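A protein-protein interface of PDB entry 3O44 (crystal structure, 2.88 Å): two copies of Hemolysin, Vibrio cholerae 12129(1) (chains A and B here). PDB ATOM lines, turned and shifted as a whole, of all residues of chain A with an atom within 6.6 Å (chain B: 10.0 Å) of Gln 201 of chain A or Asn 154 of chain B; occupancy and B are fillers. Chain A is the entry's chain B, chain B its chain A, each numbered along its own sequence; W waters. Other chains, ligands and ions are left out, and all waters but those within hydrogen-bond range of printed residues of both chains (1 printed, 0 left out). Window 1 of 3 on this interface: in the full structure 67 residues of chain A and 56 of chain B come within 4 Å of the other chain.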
ATOM      1  N   ILE A 153     -29.174 -14.363  21.247  1.00  0.00           N
ATOM      2  CA  ILE A 153     -30.296 -14.482  22.171  1.00  0.00           C
ATOM      3  C   ILE A 153     -30.011 -13.754  23.487  1.00  0.00           C
ATOM      4  O   ILE A 153     -28.946 -13.900  24.098  1.00  0.00           O
ATOM      5  CB  ILE A 153     -30.631 -15.966  22.439  1.00  0.00           C
ATOM      6  CG1 ILE A 153     -29.348 -16.811  22.280  1.00  0.00           C
ATOM      7  CG2 ILE A 153     -31.672 -16.463  21.441  1.00  0.00           C
ATOM      8  CD1 ILE A 153     -29.331 -18.175  23.012  1.00  0.00           C
ATOM      9  N   GLU A 155     -30.936 -14.205  26.793  1.00  0.00           N
ATOM     10  CA  GLU A 155     -31.572 -15.327  27.484  1.00  0.00           C
ATOM     11  C   GLU A 155     -32.407 -14.903  28.671  1.00  0.00           C
ATOM     12  O   GLU A 155     -31.981 -14.045  29.432  1.00  0.00           O
ATOM     13  CB  GLU A 155     -30.522 -16.350  27.934  1.00  0.00           C
ATOM     14  CG  GLU A 155     -30.112 -17.349  26.857  1.00  0.00           C
ATOM     15  CD  GLU A 155     -31.232 -18.302  26.458  1.00  0.00           C
ATOM     16  OE1 GLU A 155     -32.248 -18.402  27.193  1.00  0.00           O
ATOM     17  OE2 GLU A 155     -31.077 -18.967  25.412  1.00  0.00           O
ATOM     18  N   ASN A 199     -32.150 -22.200  29.567  1.00  0.00           N
ATOM     19  CA  ASN A 199     -32.131 -23.088  28.414  1.00  0.00           C
ATOM     20  C   ASN A 199     -30.811 -23.106  27.691  1.00  0.00           C
ATOM     21  O   ASN A 199     -30.092 -22.102  27.658  1.00  0.00           O
ATOM     22  CB  ASN A 199     -33.204 -22.682  27.398  1.00  0.00           C
ATOM     23  CG  ASN A 199     -34.599 -22.898  27.904  1.00  0.00           C
ATOM     24  OD1 ASN A 199     -34.949 -23.988  28.380  1.00  0.00           O
ATOM     25  ND2 ASN A 199     -35.420 -21.861  27.790  1.00  0.00           N
ATOM     26  N   THR A 200     -30.515 -24.252  27.084  1.00  0.00           N
ATOM     27  CA  THR A 200     -29.387 -24.370  26.171  1.00  0.00           C
ATOM     28  C   THR A 200     -29.833 -25.112  24.920  1.00  0.00           C
ATOM     29  O   THR A 200     -30.925 -25.695  24.886  1.00  0.00           O
ATOM     30  CB  THR A 200     -28.221 -25.130  26.801  1.00  0.00           C
ATOM     31  OG1 THR A 200     -28.658 -26.443  27.167  1.00  0.00           O
ATOM     32  CG2 THR A 200     -27.718 -24.415  28.032  1.00  0.00           C
ATOM     33  N   GLN A 201     -28.987 -25.090  23.896  1.00  0.00           N
ATOM     34  CA  GLN A 201     -29.264 -25.835  22.676  1.00  0.00           C
ATOM     35  C   GLN A 201     -28.137 -26.793  22.335  1.00  0.00           C
ATOM     36  O   GLN A 201     -27.031 -26.691  22.855  1.00  0.00           O
ATOM     37  CB  GLN A 201     -29.446 -24.879  21.513  1.00  0.00           C
ATOM     38  CG  GLN A 201     -30.533 -23.845  21.721  1.00  0.00           C
ATOM     39  CD  GLN A 201     -30.553 -22.818  20.613  1.00  0.00           C
ATOM     40  OE1 GLN A 201     -29.796 -21.840  20.632  1.00  0.00           O
ATOM     41  NE2 GLN A 201     -31.412 -23.035  19.635  1.00  0.00           N
ATOM     42  N   ASP A 202     -28.423 -27.736  21.451  1.00  0.00           N
ATOM     43  CA  ASP A 202     -27.384 -28.586  20.918  1.00  0.00           C
ATOM     44  C   ASP A 202     -26.367 -27.654  20.266  1.00  0.00           C
ATOM     45  O   ASP A 202     -25.185 -27.624  20.643  1.00  0.00           O
ATOM     46  CB  ASP A 202     -27.994 -29.538  19.897  1.00  0.00           C
ATOM     47  CG  ASP A 202     -27.085 -30.699  19.565  1.00  0.00           C
ATOM     48  OD1 ASP A 202     -27.410 -31.428  18.611  1.00  0.00           O
ATOM     49  OD2 ASP A 202     -26.058 -30.889  20.252  1.00  0.00           O
ATOM     50  N   TYR A 203     -26.844 -26.867  19.301  1.00  0.00           N
ATOM     51  CA  TYR A 203     -26.032 -25.817  18.689  1.00  0.00           C
ATOM     52  C   TYR A 203     -26.659 -24.456  18.947  1.00  0.00           C
ATOM     53  O   TYR A 203     -27.859 -24.288  18.795  1.00  0.00           O
ATOM     54  CB  TYR A 203     -25.868 -26.045  17.185  1.00  0.00           C
ATOM     55  CG  TYR A 203     -24.964 -27.204  16.862  1.00  0.00           C
ATOM     56  CD1 TYR A 203     -25.394 -28.519  17.024  1.00  0.00           C
ATOM     57  CD2 TYR A 203     -23.673 -26.988  16.401  1.00  0.00           C
ATOM     58  CE1 TYR A 203     -24.556 -29.582  16.744  1.00  0.00           C
ATOM     59  CE2 TYR A 203     -22.825 -28.055  16.107  1.00  0.00           C
ATOM     60  CZ  TYR A 203     -23.272 -29.340  16.286  1.00  0.00           C
ATOM     61  OH  TYR A 203     -22.444 -30.381  15.996  1.00  0.00           O
ATOM     62  N   ARG A 204     -25.832 -23.492  19.329  1.00  0.00           N
ATOM     63  CA  ARG A 204     -26.273 -22.130  19.569  1.00  0.00           C
ATOM     64  C   ARG A 204     -25.824 -21.247  18.421  1.00  0.00           C
ATOM     65  O   ARG A 204     -24.665 -21.303  18.011  1.00  0.00           O
ATOM     66  CB  ARG A 204     -25.679 -21.609  20.878  1.00  0.00           C
ATOM     67  CG  ARG A 204     -25.949 -20.147  21.150  1.00  0.00           C
ATOM     68  CD  ARG A 204     -25.512 -19.745  22.543  1.00  0.00           C
ATOM     69  NE  ARG A 204     -24.062 -19.809  22.709  1.00  0.00           N
ATOM     70  CZ  ARG A 204     -23.422 -19.442  23.816  1.00  0.00           C
ATOM     71  NH1 ARG A 204     -24.088 -18.974  24.868  1.00  0.00           N
ATOM     72  NH2 ARG A 204     -22.105 -19.536  23.873  1.00  0.00           N
ATOM     73  N   ILE A 205     -26.728 -20.428  17.891  1.00  0.00           N
ATOM     74  CA  ILE A 205     -26.342 -19.571  16.772  1.00  0.00           C
ATOM     75  C   ILE A 205     -25.658 -18.317  17.266  1.00  0.00           C
ATOM     76  O   ILE A 205     -26.297 -17.449  17.831  1.00  0.00           O
ATOM     77  CB  ILE A 205     -27.523 -19.180  15.903  1.00  0.00           C
ATOM     78  CG1 ILE A 205     -28.265 -20.423  15.463  1.00  0.00           C
ATOM     79  CG2 ILE A 205     -27.043 -18.421  14.693  1.00  0.00           C
ATOM     80  CD1 ILE A 205     -29.453 -20.122  14.651  1.00  0.00           C
ATOM     81  N   TRP A 219     -22.976 -21.724  14.038  1.00  0.00           N
ATOM     82  CA  TRP A 219     -23.715 -22.699  14.827  1.00  0.00           C
ATOM     83  C   TRP A 219     -22.668 -23.438  15.638  1.00  0.00           C
ATOM     84  O   TRP A 219     -21.909 -24.246  15.105  1.00  0.00           O
ATOM     85  CB  TRP A 219     -24.496 -23.664  13.938  1.00  0.00           C
ATOM     86  CG  TRP A 219     -25.847 -23.168  13.501  1.00  0.00           C
ATOM     87  CD1 TRP A 219     -27.046 -23.649  13.904  1.00  0.00           C
ATOM     88  CD2 TRP A 219     -26.126 -22.115  12.564  1.00  0.00           C
ATOM     89  NE1 TRP A 219     -28.059 -22.967  13.283  1.00  0.00           N
ATOM     90  CE2 TRP A 219     -27.523 -22.017  12.461  1.00  0.00           C
ATOM     91  CE3 TRP A 219     -25.332 -21.256  11.807  1.00  0.00           C
ATOM     92  CZ2 TRP A 219     -28.154 -21.083  11.630  1.00  0.00           C
ATOM     93  CZ3 TRP A 219     -25.953 -20.331  10.987  1.00  0.00           C
ATOM     94  CH2 TRP A 219     -27.360 -20.256  10.903  1.00  0.00           C
ATOM     95  N   ASN A 220     -22.614 -23.131  16.925  1.00  0.00           N
ATOM     96  CA  ASN A 220     -21.569 -23.621  17.799  1.00  0.00           C
ATOM     97  C   ASN A 220     -22.133 -24.593  18.828  1.00  0.00           C
ATOM     98  O   ASN A 220     -23.190 -24.343  19.381  1.00  0.00           O
ATOM     99  CB  ASN A 220     -20.915 -22.432  18.485  1.00  0.00           C
ATOM    100  CG  ASN A 220     -19.625 -22.796  19.204  1.00  0.00           C
ATOM    101  OD1 ASN A 220     -19.080 -23.907  19.045  1.00  0.00           O
ATOM    102  ND2 ASN A 220     -19.115 -21.847  19.998  1.00  0.00           N
ATOM    103  N   ARG A 221     -21.454 -25.709  19.079  1.00  0.00           N
ATOM    104  CA  ARG A 221     -21.978 -26.668  20.046  1.00  0.00           C
ATOM    105  C   ARG A 221     -22.119 -25.954  21.378  1.00  0.00           C
ATOM    106  O   ARG A 221     -21.275 -25.116  21.717  1.00  0.00           O
ATOM    107  CB  ARG A 221     -21.068 -27.896  20.158  1.00  0.00           C
ATOM    108  CG  ARG A 221     -20.992 -28.725  18.888  1.00  0.00           C
ATOM    109  CD  ARG A 221     -20.179 -29.962  19.103  1.00  0.00           C
ATOM    110  NE  ARG A 221     -20.796 -30.867  20.059  1.00  0.00           N
ATOM    111  CZ  ARG A 221     -21.777 -31.720  19.765  1.00  0.00           C
ATOM    112  NH1 ARG A 221     -22.272 -31.775  18.543  1.00  0.00           N
ATOM    113  NH2 ARG A 221     -22.279 -32.514  20.699  1.00  0.00           N
ATOM    114  N   GLN A 222     -23.194 -26.238  22.116  1.00  0.00           N
ATOM    115  CA  GLN A 222     -23.365 -25.644  23.449  1.00  0.00           C
ATOM    116  C   GLN A 222     -23.474 -26.693  24.565  1.00  0.00           C
ATOM    117  O   GLN A 222     -22.533 -26.917  25.336  1.00  0.00           O
ATOM    118  CB  GLN A 222     -24.576 -24.725  23.478  1.00  0.00           C
ATOM    119  CG  GLN A 222     -24.616 -23.835  24.712  1.00  0.00           C
ATOM    120  CD  GLN A 222     -25.868 -22.977  24.835  1.00  0.00           C
ATOM    121  OE1 GLN A 222     -26.934 -23.263  24.268  1.00  0.00           O
ATOM    122  NE2 GLN A 222     -25.737 -21.919  25.601  1.00  0.00           N
ATOM    123  N   GLN A 223     -24.636 -27.323  24.655  1.00  0.00           N
ATOM    124  CA  GLN A 223     -24.799 -28.498  25.504  1.00  0.00           C
ATOM    125  C   GLN A 223     -23.924 -29.519  24.862  1.00  0.00           C
ATOM    126  O   GLN A 223     -23.860 -29.576  23.639  1.00  0.00           O
ATOM    127  CB  GLN A 223     -26.237 -28.989  25.426  1.00  0.00           C
ATOM    128  CG  GLN A 223     -26.526 -30.138  26.312  1.00  0.00           C
ATOM    129  CD  GLN A 223     -26.766 -29.703  27.728  1.00  0.00           C
ATOM    130  OE1 GLN A 223     -26.784 -30.519  28.645  1.00  0.00           O
ATOM    131  NE2 GLN A 223     -26.968 -28.402  27.919  1.00  0.00           N
ATOM    132  N   TYR A 224     -23.237 -30.341  25.638  1.00  0.00           N
ATOM    133  CA  TYR A 224     -22.407 -31.398  25.017  1.00  0.00           C
ATOM    134  C   TYR A 224     -21.336 -30.869  24.041  1.00  0.00           C
ATOM    135  O   TYR A 224     -21.127 -31.438  22.980  1.00  0.00           O
ATOM    136  CB  TYR A 224     -23.294 -32.423  24.288  1.00  0.00           C
ATOM    137  CG  TYR A 224     -24.393 -33.022  25.146  1.00  0.00           C
ATOM    138  CD1 TYR A 224     -24.205 -33.249  26.510  1.00  0.00           C
ATOM    139  CD2 TYR A 224     -25.609 -33.385  24.589  1.00  0.00           C
ATOM    140  CE1 TYR A 224     -25.206 -33.811  27.294  1.00  0.00           C
ATOM    141  CE2 TYR A 224     -26.615 -33.948  25.360  1.00  0.00           C
ATOM    142  CZ  TYR A 224     -26.409 -34.154  26.714  1.00  0.00           C
ATOM    143  OH  TYR A 224     -27.405 -34.718  27.487  1.00  0.00           O
ATOM    144  N   LEU A 253     -27.539 -33.985  13.850  1.00  0.00           N
ATOM    145  CA  LEU A 253     -27.267 -32.631  13.418  1.00  0.00           C
ATOM    146  C   LEU A 253     -25.781 -32.332  13.497  1.00  0.00           C
ATOM    147  O   LEU A 253     -25.303 -31.372  12.898  1.00  0.00           O
ATOM    148  CB  LEU A 253     -28.023 -31.662  14.296  1.00  0.00           C
ATOM    149  CG  LEU A 253     -27.892 -30.187  13.953  1.00  0.00           C
ATOM    150  CD1 LEU A 253     -28.461 -29.933  12.588  1.00  0.00           C
ATOM    151  CD2 LEU A 253     -28.631 -29.371  15.007  1.00  0.00           C
ATOM    152  N   VAL B 150     -36.805 -29.826   7.030  1.00  0.00           N
ATOM    153  CA  VAL B 150     -35.680 -29.128   6.431  1.00  0.00           C
ATOM    154  C   VAL B 150     -34.379 -29.664   6.959  1.00  0.00           C
ATOM    155  O   VAL B 150     -33.376 -29.640   6.261  1.00  0.00           O
ATOM    156  CB  VAL B 150     -35.731 -27.596   6.663  1.00  0.00           C
ATOM    157  CG1 VAL B 150     -37.159 -27.091   6.540  1.00  0.00           C
ATOM    158  CG2 VAL B 150     -35.158 -27.236   8.016  1.00  0.00           C
ATOM    159  N   ASP B 151     -34.398 -30.155   8.190  1.00  0.00           N
ATOM    160  CA  ASP B 151     -33.175 -30.582   8.856  1.00  0.00           C
ATOM    161  C   ASP B 151     -33.431 -31.464  10.075  1.00  0.00           C
ATOM    162  O   ASP B 151     -34.565 -31.753  10.447  1.00  0.00           O
ATOM    163  CB  ASP B 151     -32.366 -29.358   9.294  1.00  0.00           C
ATOM    164  CG  ASP B 151     -30.875 -29.665   9.469  1.00  0.00           C
ATOM    165  OD1 ASP B 151     -30.421 -30.793   9.117  1.00  0.00           O
ATOM    166  OD2 ASP B 151     -30.149 -28.759   9.954  1.00  0.00           O
ATOM    167  N   ASN B 152     -32.341 -31.902  10.686  1.00  0.00           N
ATOM    168  CA  ASN B 152     -32.392 -32.520  11.998  1.00  0.00           C
ATOM    169  C   ASN B 152     -32.764 -31.470  13.058  1.00  0.00           C
ATOM    170  O   ASN B 152     -32.480 -30.268  12.902  1.00  0.00           O
ATOM    171  CB  ASN B 152     -31.044 -33.170  12.335  1.00  0.00           C
ATOM    172  CG  ASN B 152     -30.758 -34.392  11.481  1.00  0.00           C
ATOM    173  OD1 ASN B 152     -31.405 -35.432  11.636  1.00  0.00           O
ATOM    174  ND2 ASN B 152     -29.785 -34.274  10.575  1.00  0.00           N
ATOM    175  N   ILE B 153     -33.404 -31.929  14.132  1.00  0.00           N
ATOM    176  CA  ILE B 153     -33.796 -31.067  15.240  1.00  0.00           C
ATOM    177  C   ILE B 153     -32.596 -30.511  16.008  1.00  0.00           C
ATOM    178  O   ILE B 153     -31.695 -31.237  16.413  1.00  0.00           O
ATOM    179  CB  ILE B 153     -34.723 -31.818  16.200  1.00  0.00           C
ATOM    180  CG1 ILE B 153     -34.385 -33.315  16.153  1.00  0.00           C
ATOM    181  CG2 ILE B 153     -36.157 -31.664  15.762  1.00  0.00           C
ATOM    182  CD1 ILE B 153     -34.828 -34.140  17.362  1.00  0.00           C
ATOM    183  N   ASN B 154     -32.570 -29.204  16.189  1.00  0.00           N
ATOM    184  CA  ASN B 154     -31.590 -28.604  17.069  1.00  0.00           C
ATOM    185  C   ASN B 154     -32.243 -28.565  18.438  1.00  0.00           C
ATOM    186  O   ASN B 154     -32.953 -27.617  18.759  1.00  0.00           O
ATOM    187  CB  ASN B 154     -31.247 -27.207  16.578  1.00  0.00           C
ATOM    188  CG  ASN B 154     -30.157 -26.547  17.392  1.00  0.00           C
ATOM    189  OD1 ASN B 154     -29.522 -27.173  18.230  1.00  0.00           O
ATOM    190  ND2 ASN B 154     -29.936 -25.262  17.141  1.00  0.00           N
ATOM    191  N   GLU B 155     -32.041 -29.620  19.225  1.00  0.00           N
ATOM    192  CA  GLU B 155     -32.775 -29.798  20.488  1.00  0.00           C
ATOM    193  C   GLU B 155     -32.548 -28.693  21.525  1.00  0.00           C
ATOM    194  O   GLU B 155     -31.422 -28.244  21.742  1.00  0.00           O
ATOM    195  CB  GLU B 155     -32.454 -31.152  21.127  1.00  0.00           C
ATOM    196  CG  GLU B 155     -33.222 -32.328  20.550  1.00  0.00           C
ATOM    197  CD  GLU B 155     -34.716 -32.265  20.839  1.00  0.00           C
ATOM    198  OE1 GLU B 155     -35.127 -31.446  21.701  1.00  0.00           O
ATOM    199  OE2 GLU B 155     -35.481 -33.039  20.212  1.00  0.00           O
ATOM    200  N   LYS B 156     -33.621 -28.259  22.172  1.00  0.00           N
ATOM    201  CA  LYS B 156     -33.480 -27.342  23.293  1.00  0.00           C
ATOM    202  C   LYS B 156     -33.398 -28.170  24.578  1.00  0.00           C
ATOM    203  O   LYS B 156     -33.935 -29.281  24.650  1.00  0.00           O
ATOM    204  CB  LYS B 156     -34.630 -26.313  23.339  1.00  0.00           C
ATOM    205  N   PHE B 157     -32.685 -27.645  25.569  1.00  0.00           N
ATOM    206  CA  PHE B 157     -32.559 -28.307  26.868  1.00  0.00           C
ATOM    207  C   PHE B 157     -32.864 -27.337  27.989  1.00  0.00           C
ATOM    208  O   PHE B 157     -32.560 -26.144  27.886  1.00  0.00           O
ATOM    209  CB  PHE B 157     -31.146 -28.774  27.098  1.00  0.00           C
ATOM    210  CG  PHE B 157     -30.644 -29.746  26.089  1.00  0.00           C
ATOM    211  CD1 PHE B 157     -30.069 -29.298  24.908  1.00  0.00           C
ATOM    212  CD2 PHE B 157     -30.680 -31.109  26.343  1.00  0.00           C
ATOM    213  CE1 PHE B 157     -29.563 -30.199  23.979  1.00  0.00           C
ATOM    214  CE2 PHE B 157     -30.183 -32.010  25.430  1.00  0.00           C
ATOM    215  CZ  PHE B 157     -29.625 -31.554  24.240  1.00  0.00           C
ATOM    216  N   GLU B 158     -33.452 -27.843  29.068  1.00  0.00           N
ATOM    217  CA  GLU B 158     -33.699 -27.011  30.233  1.00  0.00           C
ATOM    218  C   GLU B 158     -32.804 -27.456  31.372  1.00  0.00           C
ATOM    219  O   GLU B 158     -32.919 -28.590  31.856  1.00  0.00           O
ATOM    220  CB  GLU B 158     -35.159 -27.059  30.659  1.00  0.00           C
ATOM    221  CG  GLU B 158     -35.396 -26.409  32.004  1.00  0.00           C
ATOM    222  CD  GLU B 158     -36.836 -26.505  32.458  1.00  0.00           C
ATOM    223  OE1 GLU B 158     -37.141 -27.322  33.369  1.00  0.00           O
ATOM    224  OE2 GLU B 158     -37.660 -25.755  31.895  1.00  0.00           O
ATOM    225  N   ARG B 159     -31.908 -26.558  31.782  1.00  0.00           N
ATOM    226  CA  ARG B 159     -31.041 -26.788  32.929  1.00  0.00           C
ATOM    227  C   ARG B 159     -31.627 -26.134  34.173  1.00  0.00           C
ATOM    228  O   ARG B 159     -32.105 -24.999  34.112  1.00  0.00           O
ATOM    229  CB  ARG B 159     -29.662 -26.193  32.663  1.00  0.00           C
ATOM    230  CG  ARG B 159     -28.980 -26.737  31.423  1.00  0.00           C
ATOM    231  CD  ARG B 159     -27.810 -27.680  31.773  1.00  0.00           C
ATOM    232  NE  ARG B 159     -26.562 -26.948  31.944  1.00  0.00           N
ATOM    233  CZ  ARG B 159     -25.739 -26.652  30.945  1.00  0.00           C
ATOM    234  NH1 ARG B 159     -26.041 -27.045  29.717  1.00  0.00           N
ATOM    235  NH2 ARG B 159     -24.620 -25.970  31.171  1.00  0.00           N
ATOM    236  N   LEU B 196     -31.286 -31.614  34.328  1.00  0.00           N
ATOM    237  CA  LEU B 196     -31.288 -31.500  32.876  1.00  0.00           C
ATOM    238  C   LEU B 196     -32.543 -32.137  32.313  1.00  0.00           C
ATOM    239  O   LEU B 196     -32.805 -33.310  32.550  1.00  0.00           O
ATOM    240  CB  LEU B 196     -30.078 -32.185  32.277  1.00  0.00           C
ATOM    241  CG  LEU B 196     -30.082 -32.137  30.751  1.00  0.00           C
ATOM    242  CD1 LEU B 196     -29.942 -30.708  30.258  1.00  0.00           C
ATOM    243  CD2 LEU B 196     -28.983 -32.988  30.175  1.00  0.00           C
ATOM    244  N   THR B 197     -33.325 -31.360  31.569  1.00  0.00           N
ATOM    245  CA  THR B 197     -34.560 -31.876  31.000  1.00  0.00           C
ATOM    246  C   THR B 197     -34.510 -31.754  29.483  1.00  0.00           C
ATOM    247  O   THR B 197     -34.048 -30.745  28.949  1.00  0.00           O
ATOM    248  CB  THR B 197     -35.765 -31.116  31.549  1.00  0.00           C
ATOM    249  OG1 THR B 197     -35.597 -30.928  32.959  1.00  0.00           O
ATOM    250  CG2 THR B 197     -37.041 -31.880  31.293  1.00  0.00           C
ATOM    251  N   TYR B 198     -34.958 -32.793  28.789  1.00  0.00           N
ATOM    252  CA  TYR B 198     -34.997 -32.753  27.331  1.00  0.00           C
ATOM    253  C   TYR B 198     -35.988 -33.755  26.752  1.00  0.00           C
ATOM    254  O   TYR B 198     -36.567 -34.557  27.486  1.00  0.00           O
ATOM    255  CB  TYR B 198     -33.615 -32.996  26.764  1.00  0.00           C
ATOM    256  CG  TYR B 198     -33.062 -34.363  27.084  1.00  0.00           C
ATOM    257  CD1 TYR B 198     -32.349 -34.594  28.250  1.00  0.00           C
ATOM    258  CD2 TYR B 198     -33.235 -35.426  26.208  1.00  0.00           C
ATOM    259  CE1 TYR B 198     -31.821 -35.858  28.533  1.00  0.00           C
ATOM    260  CE2 TYR B 198     -32.710 -36.692  26.484  1.00  0.00           C
ATOM    261  CZ  TYR B 198     -32.003 -36.901  27.643  1.00  0.00           C
ATOM    262  OH  TYR B 198     -31.491 -38.152  27.916  1.00  0.00           O
ATOM    263  N   ASN B 199     -36.197 -33.699  25.440  1.00  0.00           N
ATOM    264  CA  ASN B 199     -37.204 -34.554  24.820  1.00  0.00           C
ATOM    265  C   ASN B 199     -36.636 -35.647  23.933  1.00  0.00           C
ATOM    266  O   ASN B 199     -35.567 -35.502  23.334  1.00  0.00           O
ATOM    267  CB  ASN B 199     -38.177 -33.726  23.986  1.00  0.00           C
ATOM    268  CG  ASN B 199     -39.011 -32.785  24.823  1.00  0.00           C
ATOM    269  OD1 ASN B 199     -39.642 -33.196  25.801  1.00  0.00           O
ATOM    270  ND2 ASN B 199     -39.027 -31.509  24.440  1.00  0.00           N
ATOM    271  N   GLN B 201     -38.235 -38.979  21.120  1.00  0.00           N
ATOM    272  CA  GLN B 201     -39.409 -39.501  20.440  1.00  0.00           C
ATOM    273  C   GLN B 201     -39.348 -41.015  20.341  1.00  0.00           C
ATOM    274  O   GLN B 201     -38.292 -41.624  20.538  1.00  0.00           O
ATOM    275  CB  GLN B 201     -39.520 -38.911  19.045  1.00  0.00           C
ATOM    276  CG  GLN B 201     -39.543 -37.425  18.996  1.00  0.00           C
ATOM    277  CD  GLN B 201     -39.501 -36.916  17.580  1.00  0.00           C
ATOM    278  OE1 GLN B 201     -38.418 -36.781  16.979  1.00  0.00           O
ATOM    279  NE2 GLN B 201     -40.688 -36.649  17.015  1.00  0.00           N
ATOM    280  N   ARG B 204     -37.211 -40.903  15.781  1.00  0.00           N
ATOM    281  CA  ARG B 204     -36.618 -39.613  15.496  1.00  0.00           C
ATOM    282  C   ARG B 204     -36.309 -39.529  14.014  1.00  0.00           C
ATOM    283  O   ARG B 204     -35.689 -40.428  13.458  1.00  0.00           O
ATOM    284  CB  ARG B 204     -35.319 -39.463  16.281  1.00  0.00           C
ATOM    285  CG  ARG B 204     -34.535 -38.233  15.902  1.00  0.00           C
ATOM    286  CD  ARG B 204     -33.386 -37.986  16.855  1.00  0.00           C
ATOM    287  NE  ARG B 204     -32.359 -39.013  16.745  1.00  0.00           N
ATOM    288  CZ  ARG B 204     -31.218 -39.006  17.431  1.00  0.00           C
ATOM    289  NH1 ARG B 204     -30.964 -38.025  18.279  1.00  0.00           N
ATOM    290  NH2 ARG B 204     -30.330 -39.980  17.280  1.00  0.00           N
ATOM    291  N   ILE B 205     -36.730 -38.453  13.360  1.00  0.00           N
ATOM    292  CA  ILE B 205     -36.468 -38.341  11.933  1.00  0.00           C
ATOM    293  C   ILE B 205     -35.036 -37.880  11.694  1.00  0.00           C
ATOM    294  O   ILE B 205     -34.701 -36.726  11.960  1.00  0.00           O
ATOM    295  CB  ILE B 205     -37.425 -37.388  11.257  1.00  0.00           C
ATOM    296  CG1 ILE B 205     -38.857 -37.838  11.511  1.00  0.00           C
ATOM    297  CG2 ILE B 205     -37.173 -37.360   9.771  1.00  0.00           C
ATOM    298  CD1 ILE B 205     -39.903 -36.899  10.949  1.00  0.00           C
HETATM  299  O   HOH W   1     -32.853 -25.088  19.257  1.00  0.00           O
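OE1 of Gln 222 of chain A sits at hydrogen-bond distance from N of Gln 201 of chain A (2.8 Å).
The backbone carbonyl oxygen of Gln 201 of chain A is in hydrogen-bond range of the backbone NH of Gln 223 of chain A (3.1 Å).
The side-chain hydroxyl (OH) of Tyr 203 of chain A sits at hydrogen-bond distance from the guanidinium group (NH1) of Arg 221 of chain A (2.9 Å).
Gln 201 of chain A touches just these residues of chain B: Asn 154 (3.7 Å) and Glu 155 (3.4 Å).
Asn 154 of chain B touches just these residues of chain A: Gln 201 (3.7 Å), Asp 202 (3.3 Å), Tyr 203 (2.8 Å) and Leu 253 (3.7 Å).
Asp 202 of chain A touches just these residues of chain B: Asn 154, Glu 155 and Phe 157.
No residue of chain B comes within 4 Å of Gln 222 of chain A.
Of the printed residues of chain A, Glu 158 of chain B touches Asn 199.
Printed residues of chain A within 4 Å of Ile 153 of chain B: Leu 253.
Printed residues of chain B within 4 Å of Gln 223 of chain A: Phe 157 (3.8 Å), Arg 159 (2.4 Å) and Leu 196 (3.6 Å).
Of the printed residues of chain A, Arg 159 of chain B touches Thr 200 and Gln 223.
Arg 204 of chain A touches none of the printed residues of chain B.
The nearest residue of chain B that does not touch Gln 201 of chain A is Phe 157 of chain B (4.04 Å).
The nearest residue of chain A that does not touch Asn 154 of chain B is Trp 219 of chain A (4.6 Å).
Of the 17 printed residues of chain B, 10 touch a printed residue of chain A.
Printed residues of chain B that touch a printed residue of chain A: Asp 151, Asn 152, Ile 153, Asn 154, Glu 155, Lys 156, Phe 157, Glu 158, Arg 159 and Leu 196.
Hydrophobic or aromatic side chains of chain B that line the printed part of chain A: Phe 157 and Leu 196.
Of the 16 printed residues of chain A, 8 touch a printed residue of chain B.
Among the printed residues, 19 pairs touch across the chains.
Water W1 lies within hydrogen-bond range of NE2 of Gln 201 of chain A (2.5 Å) and O of Asn 154 of chain B (2.6 Å).
The backbone NH (N) of Asp 202 of chain A sits close to the side-chain amide oxygen (OD1) of Asn 154 of chain B, 3.4 Å away.
O of Tyr 203 of chain A lies within hydrogen-bond range of ND2 of Asn 154 of chain B (2.8 Å).
The backbone carbonyl oxygen (O) of Glu 155 of chain B is in hydrogen-bond range of the backbone NH (N) of Asp 202 of chain A.
OD1 of Asn 199 of chain A sits close to O of Phe 157 of chain B (3.3 Å).
The backbone NH of Phe 157 of chain B is in hydrogen-bond range of the backbone carbonyl oxygen of Thr 200 of chain A, at 2.7 Å.
The side-chain amide nitrogen (NE2) of Gln 223 of chain A sits close to the guanidinium group (NH1) of Arg 159 of chain B, 2.4 Å away.
Among the printed residues, merely in contact across the chains: Leu 253 of chain A with Asp 151 of chain B (3.3 Å), Gln 201 of chain A with Glu 155 of chain B (3.4 Å), Thr 200 of chain A with Lys 156 of chain B (3.4 Å), Thr 200 of chain A with Arg 159 of chain B (3.5 Å), Gln 223 of chain A with Leu 196 of chain B (3.6 Å), Tyr 224 of chain A with Leu 196 of chain B (3.6 Å), Gln 201 of chain A with Asn 154 of chain B (3.7 Å), Leu 253 of chain A with Asn 154 of chain B (3.7 Å), Asp 202 of chain A with Phe 157 of chain B (3.7 Å), Asn 199 of chain A with Glu 158 of chain B (3.8 Å), Gln 223 of chain A with Phe 157 of chain B (3.8 Å), Leu 253 of chain A with Ile 153 of chain B (3.9 Å) and Leu 253 of chain A with Asn 152 of chain B (3.9 Å).
Gln 201 of chain A touches Glu 155 of chain B, but with the chains exchanged Glu 155 of chain A does not touch Gln 201 of chain B (21.0 Å).
Of the 19 pairs that touch across the chains among the printed residues, none has its exchanged pair printed and touching as well.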
